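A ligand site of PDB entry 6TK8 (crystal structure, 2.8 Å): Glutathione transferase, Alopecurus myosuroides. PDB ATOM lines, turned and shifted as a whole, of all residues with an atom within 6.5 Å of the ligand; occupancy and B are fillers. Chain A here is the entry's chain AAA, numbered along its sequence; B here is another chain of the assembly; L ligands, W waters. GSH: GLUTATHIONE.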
ATOM      1  N   SER A  12     -22.257  18.854  -7.988  1.00  0.00           N
ATOM      2  CA  SER A  12     -22.561  18.122  -9.243  1.00  0.00           C
ATOM      3  C   SER A  12     -23.168  19.053 -10.319  1.00  0.00           C
ATOM      4  O   SER A  12     -24.067  19.870 -10.002  1.00  0.00           O
ATOM      5  CB  SER A  12     -23.448  16.927  -8.950  1.00  0.00           C
ATOM      6  OG  SER A  12     -24.258  16.603 -10.073  1.00  0.00           O
ATOM      7  N   ASN A  14     -24.813  17.974 -13.327  1.00  0.00           N
ATOM      8  CA  ASN A  14     -26.164  17.511 -13.725  1.00  0.00           C
ATOM      9  C   ASN A  14     -27.175  17.897 -12.635  1.00  0.00           C
ATOM     10  O   ASN A  14     -28.394  17.827 -12.926  1.00  0.00           O
ATOM     11  CB  ASN A  14     -26.199  16.012 -14.064  1.00  0.00           C
ATOM     12  CG  ASN A  14     -25.602  15.749 -15.438  1.00  0.00           C
ATOM     13  OD1 ASN A  14     -26.275  15.221 -16.326  1.00  0.00           O
ATOM     14  ND2 ASN A  14     -24.379  16.184 -15.646  1.00  0.00           N
ATOM     15  N   ARG A  17     -27.860  21.748 -13.133  1.00  0.00           N
ATOM     16  CA  ARG A  17     -28.862  21.782 -14.244  1.00  0.00           C
ATOM     17  C   ARG A  17     -30.265  21.904 -13.635  1.00  0.00           C
ATOM     18  O   ARG A  17     -30.919  22.919 -13.880  1.00  0.00           O
ATOM     19  CB  ARG A  17     -28.695  20.556 -15.159  1.00  0.00           C
ATOM     20  CG  ARG A  17     -29.650  20.478 -16.351  1.00  0.00           C
ATOM     21  CD  ARG A  17     -29.372  19.282 -17.281  1.00  0.00           C
ATOM     22  NE  ARG A  17     -28.445  19.602 -18.357  1.00  0.00           N
ATOM     23  CZ  ARG A  17     -27.141  19.311 -18.360  1.00  0.00           C
ATOM     24  NH1 ARG A  17     -26.587  18.663 -17.359  1.00  0.00           N
ATOM     25  NH2 ARG A  17     -26.383  19.690 -19.382  1.00  0.00           N
ATOM     26  N   PHE A  36     -20.898   9.787  -2.690  1.00  0.00           N
ATOM     27  CA  PHE A  36     -20.236   8.875  -3.661  1.00  0.00           C
ATOM     28  C   PHE A  36     -19.191   7.996  -2.978  1.00  0.00           C
ATOM     29  O   PHE A  36     -18.965   6.878  -3.460  1.00  0.00           O
ATOM     30  CB  PHE A  36     -19.537   9.671  -4.766  1.00  0.00           C
ATOM     31  CG  PHE A  36     -20.442  10.123  -5.868  1.00  0.00           C
ATOM     32  CD1 PHE A  36     -21.509   9.338  -6.273  1.00  0.00           C
ATOM     33  CD2 PHE A  36     -20.190  11.315  -6.530  1.00  0.00           C
ATOM     34  CE1 PHE A  36     -22.333   9.747  -7.308  1.00  0.00           C
ATOM     35  CE2 PHE A  36     -21.018  11.715  -7.566  1.00  0.00           C
ATOM     36  CZ  PHE A  36     -22.085  10.928  -7.950  1.00  0.00           C
ATOM     37  N   HIS A  41     -25.256   6.019  -3.975  1.00  0.00           N
ATOM     38  CA  HIS A  41     -25.989   6.106  -5.270  1.00  0.00           C
ATOM     39  C   HIS A  41     -26.249   4.706  -5.833  1.00  0.00           C
ATOM     40  O   HIS A  41     -27.071   4.587  -6.756  1.00  0.00           O
ATOM     41  CB  HIS A  41     -25.227   6.964  -6.278  1.00  0.00           C
ATOM     42  CG  HIS A  41     -23.898   6.434  -6.644  1.00  0.00           C
ATOM     43  ND1 HIS A  41     -22.818   6.521  -5.782  1.00  0.00           N
ATOM     44  CD2 HIS A  41     -23.446   5.849  -7.778  1.00  0.00           C
ATOM     45  CE1 HIS A  41     -21.750   6.007  -6.370  1.00  0.00           C
ATOM     46  NE2 HIS A  41     -22.109   5.571  -7.599  1.00  0.00           N
ATOM     47  N   LYS A  42     -25.559   3.702  -5.295  1.00  0.00           N
ATOM     48  CA  LYS A  42     -25.731   2.266  -5.670  1.00  0.00           C
ATOM     49  C   LYS A  42     -26.631   1.587  -4.637  1.00  0.00           C
ATOM     50  O   LYS A  42     -27.239   0.549  -4.969  1.00  0.00           O
ATOM     51  CB  LYS A  42     -24.342   1.655  -5.812  1.00  0.00           C
ATOM     52  CG  LYS A  42     -23.499   2.329  -6.876  1.00  0.00           C
ATOM     53  CD  LYS A  42     -24.234   2.461  -8.177  1.00  0.00           C
ATOM     54  CE  LYS A  42     -23.348   2.745  -9.377  1.00  0.00           C
ATOM     55  NZ  LYS A  42     -24.154   2.837 -10.623  1.00  0.00           N
ATOM     56  N   ASN A  50     -33.659   6.042  -9.080  1.00  0.00           N
ATOM     57  CA  ASN A  50     -32.911   5.789 -10.341  1.00  0.00           C
ATOM     58  C   ASN A  50     -32.490   4.316 -10.422  1.00  0.00           C
ATOM     59  O   ASN A  50     -31.492   3.886  -9.849  1.00  0.00           O
ATOM     60  CB  ASN A  50     -31.661   6.655 -10.480  1.00  0.00           C
ATOM     61  CG  ASN A  50     -31.143   6.640 -11.902  1.00  0.00           C
ATOM     62  OD1 ASN A  50     -31.537   5.769 -12.679  1.00  0.00           O
ATOM     63  ND2 ASN A  50     -30.269   7.560 -12.250  1.00  0.00           N
ATOM     64  N   PHE A  52     -30.670   2.952 -12.467  1.00  0.00           N
ATOM     65  CA  PHE A  52     -29.259   2.913 -12.958  1.00  0.00           C
ATOM     66  C   PHE A  52     -28.314   3.528 -11.938  1.00  0.00           C
ATOM     67  O   PHE A  52     -27.103   3.567 -12.193  1.00  0.00           O
ATOM     68  CB  PHE A  52     -29.134   3.614 -14.308  1.00  0.00           C
ATOM     69  CG  PHE A  52     -30.102   3.097 -15.330  1.00  0.00           C
ATOM     70  CD1 PHE A  52     -29.860   1.901 -15.989  1.00  0.00           C
ATOM     71  CD2 PHE A  52     -31.268   3.771 -15.611  1.00  0.00           C
ATOM     72  CE1 PHE A  52     -30.758   1.412 -16.927  1.00  0.00           C
ATOM     73  CE2 PHE A  52     -32.179   3.275 -16.540  1.00  0.00           C
ATOM     74  CZ  PHE A  52     -31.920   2.094 -17.198  1.00  0.00           C
ATOM     75  N   GLY A  53     -28.842   3.991 -10.796  1.00  0.00           N
ATOM     76  CA  GLY A  53     -28.000   4.286  -9.625  1.00  0.00           C
ATOM     77  C   GLY A  53     -26.990   5.365  -9.958  1.00  0.00           C
ATOM     78  O   GLY A  53     -25.817   5.248  -9.575  1.00  0.00           O
ATOM     79  N   GLN A  54     -27.463   6.377 -10.663  1.00  0.00           N
ATOM     80  CA  GLN A  54     -26.732   7.637 -10.921  1.00  0.00           C
ATOM     81  C   GLN A  54     -27.544   8.785 -10.342  1.00  0.00           C
ATOM     82  O   GLN A  54     -28.787   8.633 -10.239  1.00  0.00           O
ATOM     83  CB  GLN A  54     -26.594   7.830 -12.419  1.00  0.00           C
ATOM     84  CG  GLN A  54     -26.036   6.609 -13.128  1.00  0.00           C
ATOM     85  CD  GLN A  54     -25.910   6.946 -14.582  1.00  0.00           C
ATOM     86  OE1 GLN A  54     -26.914   7.169 -15.254  1.00  0.00           O
ATOM     87  NE2 GLN A  54     -24.673   7.059 -15.051  1.00  0.00           N
ATOM     88  N   ILE A  55     -26.831   9.862  -9.985  1.00  0.00           N
ATOM     89  CA  ILE A  55     -27.407  11.186  -9.578  1.00  0.00           C
ATOM     90  C   ILE A  55     -27.540  12.015 -10.849  1.00  0.00           C
ATOM     91  O   ILE A  55     -26.783  11.837 -11.792  1.00  0.00           O
ATOM     92  CB  ILE A  55     -26.559  11.846  -8.465  1.00  0.00           C
ATOM     93  CG1 ILE A  55     -25.193  12.353  -8.946  1.00  0.00           C
ATOM     94  CG2 ILE A  55     -26.371  10.924  -7.282  1.00  0.00           C
ATOM     95  CD1 ILE A  55     -25.174  13.815  -9.294  1.00  0.00           C
ATOM     96  N   PRO A  56     -28.553  12.901 -10.959  1.00  0.00           N
ATOM     97  CA  PRO A  56     -29.537  13.124  -9.904  1.00  0.00           C
ATOM     98  C   PRO A  56     -30.821  12.302 -10.063  1.00  0.00           C
ATOM     99  O   PRO A  56     -31.048  11.680 -11.107  1.00  0.00           O
ATOM    100  CB  PRO A  56     -29.821  14.611 -10.142  1.00  0.00           C
ATOM    101  CG  PRO A  56     -29.867  14.733 -11.648  1.00  0.00           C
ATOM    102  CD  PRO A  56     -28.822  13.737 -12.141  1.00  0.00           C
ATOM    103  N   TRP A  66     -35.772  10.449 -12.905  1.00  0.00           N
ATOM    104  CA  TRP A  66     -34.307  10.591 -13.118  1.00  0.00           C
ATOM    105  C   TRP A  66     -34.040  11.147 -14.531  1.00  0.00           C
ATOM    106  O   TRP A  66     -34.957  11.108 -15.387  1.00  0.00           O
ATOM    107  CB  TRP A  66     -33.519   9.306 -12.847  1.00  0.00           C
ATOM    108  CG  TRP A  66     -33.723   8.185 -13.825  1.00  0.00           C
ATOM    109  CD1 TRP A  66     -32.824   7.733 -14.741  1.00  0.00           C
ATOM    110  CD2 TRP A  66     -34.880   7.324 -13.946  1.00  0.00           C
ATOM    111  NE1 TRP A  66     -33.340   6.679 -15.446  1.00  0.00           N
ATOM    112  CE2 TRP A  66     -34.591   6.385 -14.974  1.00  0.00           C
ATOM    113  CE3 TRP A  66     -36.103   7.230 -13.285  1.00  0.00           C
ATOM    114  CZ2 TRP A  66     -35.501   5.410 -15.374  1.00  0.00           C
ATOM    115  CZ3 TRP A  66     -37.014   6.279 -13.703  1.00  0.00           C
ATOM    116  CH2 TRP A  66     -36.718   5.380 -14.726  1.00  0.00           C
ATOM    117  N   GLU A  67     -32.827  11.681 -14.700  1.00  0.00           N
ATOM    118  CA  GLU A  67     -32.236  12.168 -15.965  1.00  0.00           C
ATOM    119  C   GLU A  67     -32.453  13.690 -15.968  1.00  0.00           C
ATOM    120  O   GLU A  67     -33.559  14.150 -16.239  1.00  0.00           O
ATOM    121  CB  GLU A  67     -32.806  11.321 -17.103  1.00  0.00           C
ATOM    122  CG  GLU A  67     -31.794  11.013 -18.196  1.00  0.00           C
ATOM    123  CD  GLU A  67     -30.916   9.767 -18.060  1.00  0.00           C
ATOM    124  OE1 GLU A  67     -31.480   8.667 -17.845  1.00  0.00           O
ATOM    125  OE2 GLU A  67     -29.662   9.898 -18.226  1.00  0.00           O
ATOM    126  N   SER A  68     -31.411  14.449 -15.637  1.00  0.00           N
ATOM    127  CA  SER A  68     -31.446  15.921 -15.381  1.00  0.00           C
ATOM    128  C   SER A  68     -32.286  16.667 -16.426  1.00  0.00           C
ATOM    129  O   SER A  68     -32.960  17.619 -16.035  1.00  0.00           O
ATOM    130  CB  SER A  68     -30.047  16.510 -15.263  1.00  0.00           C
ATOM    131  OG  SER A  68     -29.204  16.168 -16.370  1.00  0.00           O
ATOM    132  N   ARG A  69     -32.271  16.290 -17.706  1.00  0.00           N
ATOM    133  CA  ARG A  69     -32.970  17.083 -18.745  1.00  0.00           C
ATOM    134  C   ARG A  69     -34.463  16.744 -18.741  1.00  0.00           C
ATOM    135  O   ARG A  69     -35.256  17.663 -18.946  1.00  0.00           O
ATOM    136  CB  ARG A  69     -32.373  16.922 -20.150  1.00  0.00           C
ATOM    137  CG  ARG A  69     -31.020  17.604 -20.334  1.00  0.00           C
ATOM    138  CD  ARG A  69     -30.270  17.105 -21.557  1.00  0.00           C
ATOM    139  NE  ARG A  69     -28.907  17.623 -21.556  1.00  0.00           N
ATOM    140  CZ  ARG A  69     -27.815  16.971 -21.163  1.00  0.00           C
ATOM    141  NH1 ARG A  69     -27.895  15.715 -20.747  1.00  0.00           N
ATOM    142  NH2 ARG A  69     -26.639  17.565 -21.217  1.00  0.00           N
ATOM    143  N   ALA A  70     -34.855  15.508 -18.467  1.00  0.00           N
ATOM    144  CA  ALA A  70     -36.290  15.140 -18.325  1.00  0.00           C
ATOM    145  C   ALA A  70     -36.860  15.797 -17.065  1.00  0.00           C
ATOM    146  O   ALA A  70     -38.001  16.261 -17.105  1.00  0.00           O
ATOM    147  CB  ALA A  70     -36.496  13.650 -18.313  1.00  0.00           C
ATOM    148  N   ILE A  71     -36.085  15.821 -15.971  1.00  0.00           N
ATOM    149  CA  ILE A  71     -36.474  16.439 -14.673  1.00  0.00           C
ATOM    150  C   ILE A  71     -36.778  17.908 -14.973  1.00  0.00           C
ATOM    151  O   ILE A  71     -37.897  18.347 -14.623  1.00  0.00           O
ATOM    152  CB  ILE A  71     -35.351  16.238 -13.635  1.00  0.00           C
ATOM    153  CG1 ILE A  71     -35.422  14.839 -13.021  1.00  0.00           C
ATOM    154  CG2 ILE A  71     -35.311  17.301 -12.553  1.00  0.00           C
ATOM    155  CD1 ILE A  71     -34.058  14.221 -12.753  1.00  0.00           C
ATOM    156  N   TYR A 175     -21.628  22.940 -16.946  1.00  0.00           N
ATOM    157  CA  TYR A 175     -20.295  22.451 -17.409  1.00  0.00           C
ATOM    158  C   TYR A 175     -19.397  23.627 -17.784  1.00  0.00           C
ATOM    159  O   TYR A 175     -18.154  23.602 -17.532  1.00  0.00           O
ATOM    160  CB  TYR A 175     -20.413  21.438 -18.548  1.00  0.00           C
ATOM    161  CG  TYR A 175     -20.651  20.019 -18.098  1.00  0.00           C
ATOM    162  CD1 TYR A 175     -19.589  19.180 -17.792  1.00  0.00           C
ATOM    163  CD2 TYR A 175     -21.927  19.516 -17.966  1.00  0.00           C
ATOM    164  CE1 TYR A 175     -19.788  17.878 -17.382  1.00  0.00           C
ATOM    165  CE2 TYR A 175     -22.161  18.209 -17.566  1.00  0.00           C
ATOM    166  CZ  TYR A 175     -21.082  17.387 -17.279  1.00  0.00           C
ATOM    167  OH  TYR A 175     -21.313  16.112 -16.887  1.00  0.00           O
ATOM    168  N   GLU B 103     -34.412   9.864 -22.747  1.00  0.00           N
ATOM    169  CA  GLU B 103     -33.048  10.228 -22.298  1.00  0.00           C
ATOM    170  C   GLU B 103     -32.294   8.998 -21.760  1.00  0.00           C
ATOM    171  O   GLU B 103     -31.076   9.049 -21.612  1.00  0.00           O
ATOM    172  CB  GLU B 103     -33.177  11.387 -21.319  1.00  0.00           C
ATOM    173  CG  GLU B 103     -31.909  12.207 -21.291  1.00  0.00           C
ATOM    174  CD  GLU B 103     -32.087  13.576 -20.675  1.00  0.00           C
ATOM    175  OE1 GLU B 103     -32.997  14.301 -21.180  1.00  0.00           O
ATOM    176  OE2 GLU B 103     -31.317  13.923 -19.721  1.00  0.00           O
ATOM    177  N   HIS B 107     -28.487   8.373 -23.385  1.00  0.00           N
ATOM    178  CA  HIS B 107     -27.370   8.488 -22.419  1.00  0.00           C
ATOM    179  C   HIS B 107     -26.928   7.139 -21.825  1.00  0.00           C
ATOM    180  O   HIS B 107     -25.847   7.097 -21.225  1.00  0.00           O
ATOM    181  CB  HIS B 107     -27.756   9.501 -21.356  1.00  0.00           C
ATOM    182  CG  HIS B 107     -27.815  10.875 -21.913  1.00  0.00           C
ATOM    183  ND1 HIS B 107     -26.727  11.711 -21.906  1.00  0.00           N
ATOM    184  CD2 HIS B 107     -28.805  11.546 -22.515  1.00  0.00           C
ATOM    185  CE1 HIS B 107     -27.055  12.843 -22.468  1.00  0.00           C
ATOM    186  NE2 HIS B 107     -28.341  12.777 -22.839  1.00  0.00           N
ATOM    187  N   THR B 108     -27.712   6.082 -21.950  1.00  0.00           N
ATOM    188  CA  THR B 108     -27.434   4.824 -21.219  1.00  0.00           C
ATOM    189  C   THR B 108     -27.439   3.634 -22.172  1.00  0.00           C
ATOM    190  O   THR B 108     -26.439   2.849 -22.144  1.00  0.00           O
ATOM    191  CB  THR B 108     -28.464   4.667 -20.110  1.00  0.00           C
ATOM    192  OG1 THR B 108     -28.318   5.870 -19.375  1.00  0.00           O
ATOM    193  CG2 THR B 108     -28.244   3.464 -19.224  1.00  0.00           C
HETATM  194  N1  GSH L   1     -26.704  12.027 -18.120  1.00  0.00           N
HETATM  195  CA1 GSH L   1     -27.607  11.659 -16.989  1.00  0.00           C
HETATM  196  C1  GSH L   1     -28.512  12.862 -16.676  1.00  0.00           C
HETATM  197  O11 GSH L   1     -28.566  13.256 -15.496  1.00  0.00           O
HETATM  198  O12 GSH L   1     -29.175  13.358 -17.642  1.00  0.00           O
HETATM  199  CB1 GSH L   1     -26.801  11.100 -15.796  1.00  0.00           C
HETATM  200  CG1 GSH L   1     -25.574  11.897 -15.339  1.00  0.00           C
HETATM  201  CD1 GSH L   1     -24.640  11.033 -14.525  1.00  0.00           C
HETATM  202  OE1 GSH L   1     -24.338   9.904 -14.897  1.00  0.00           O
HETATM  203  N2  GSH L   1     -24.206  11.519 -13.361  1.00  0.00           N
HETATM  204  CA2 GSH L   1     -22.982  11.099 -12.674  1.00  0.00           C
HETATM  205  C2  GSH L   1     -23.032   9.763 -11.903  1.00  0.00           C
HETATM  206  O2  GSH L   1     -23.987   9.479 -11.186  1.00  0.00           O
HETATM  207  CB2 GSH L   1     -22.479  12.180 -11.736  1.00  0.00           C
HETATM  208  SG2 GSH L   1     -20.712  12.100 -11.374  1.00  0.00           S
HETATM  209  N3  GSH L   1     -21.962   8.972 -12.015  1.00  0.00           N
HETATM  210  CA3 GSH L   1     -21.834   7.744 -11.253  1.00  0.00           C
HETATM  211  C3  GSH L   1     -22.391   6.524 -11.983  1.00  0.00           C
HETATM  212  O31 GSH L   1     -23.035   6.744 -13.024  1.00  0.00           O
HETATM  213  O32 GSH L   1     -22.151   5.393 -11.482  1.00  0.00           O
HETATM  214  O   HOH W   1     -23.663  14.979 -12.004  1.00  0.00           O
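The side-chain amino group (NZ) of Lys 42 lies within salt-bridge range of an oxygen (O32) of the ligand, at 3.4 Å.
An oxygen (O2) of the ligand is in hydrogen-bond range of the backbone NH (N) of Ile 55.
The backbone NH (N) of Ser 68 sits at hydrogen-bond distance from an oxygen (O11) of the ligand (3.1 Å).
A nitrogen (N2) of the ligand sits at hydrogen-bond distance from the backbone carbonyl oxygen of Ile 55 (3.0 Å).
The side-chain amide nitrogen of Gln 54 sits at hydrogen-bond distance from an oxygen (O31) of the ligand (2.6 Å).
An oxygen (O12) of the ligand is in hydrogen-bond range of the side-chain hydroxyl of Ser 68 (3.1 Å).
The side-chain carboxylate of Glu 103 of chain B sits close to an oxygen (O12) of the ligand (3.0 Å).
N1 of the ligand is in salt-bridge range of OE2 of Glu 67 (3.6 Å).
The side-chain amide oxygen of Asn 14 sits close to an oxygen (O11) of the ligand, at 3.1 Å.
NZ of Lys 42 lies within hydrogen-bond range of O of Phe 52 (3.4 Å).
ND2 of Asn 14 is in hydrogen-bond range of OH of Tyr 175, 3.3 Å away.
O of Gln 54 sits at hydrogen-bond distance from ND2 of Asn 50 (2.7 Å).
The side-chain hydroxyl (OG) of Ser 68 is in hydrogen-bond range of the side-chain amide oxygen (OD1) of Asn 14.
The backbone carbonyl oxygen (O) of Gly 53 sits at hydrogen-bond distance from the side-chain amino group (NZ) of Lys 42 (3.1 Å).
The side-chain carboxylate of Glu 103 of chain B lies within salt-bridge range of the guanidinium group of Arg 69.
Merely in contact with the ligand: Phe 36 (3.8 Å), His 41 (3.9 Å), Pro 56 (3.4 Å) and His 107 of chain B (3.8 Å).
Within 4 Å of the ligand: Asn 14, Phe 36, His 41, Lys 42, Gln 54, Ile 55, Pro 56, Glu 67, Ser 68, Glu 103 of chain B and His 107 of chain B.
The nearest printed residue that does not touch the ligand is Arg 69 (4.1 Å).
Water W1 bridges OG of Ser 12 and N of Asn 14.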
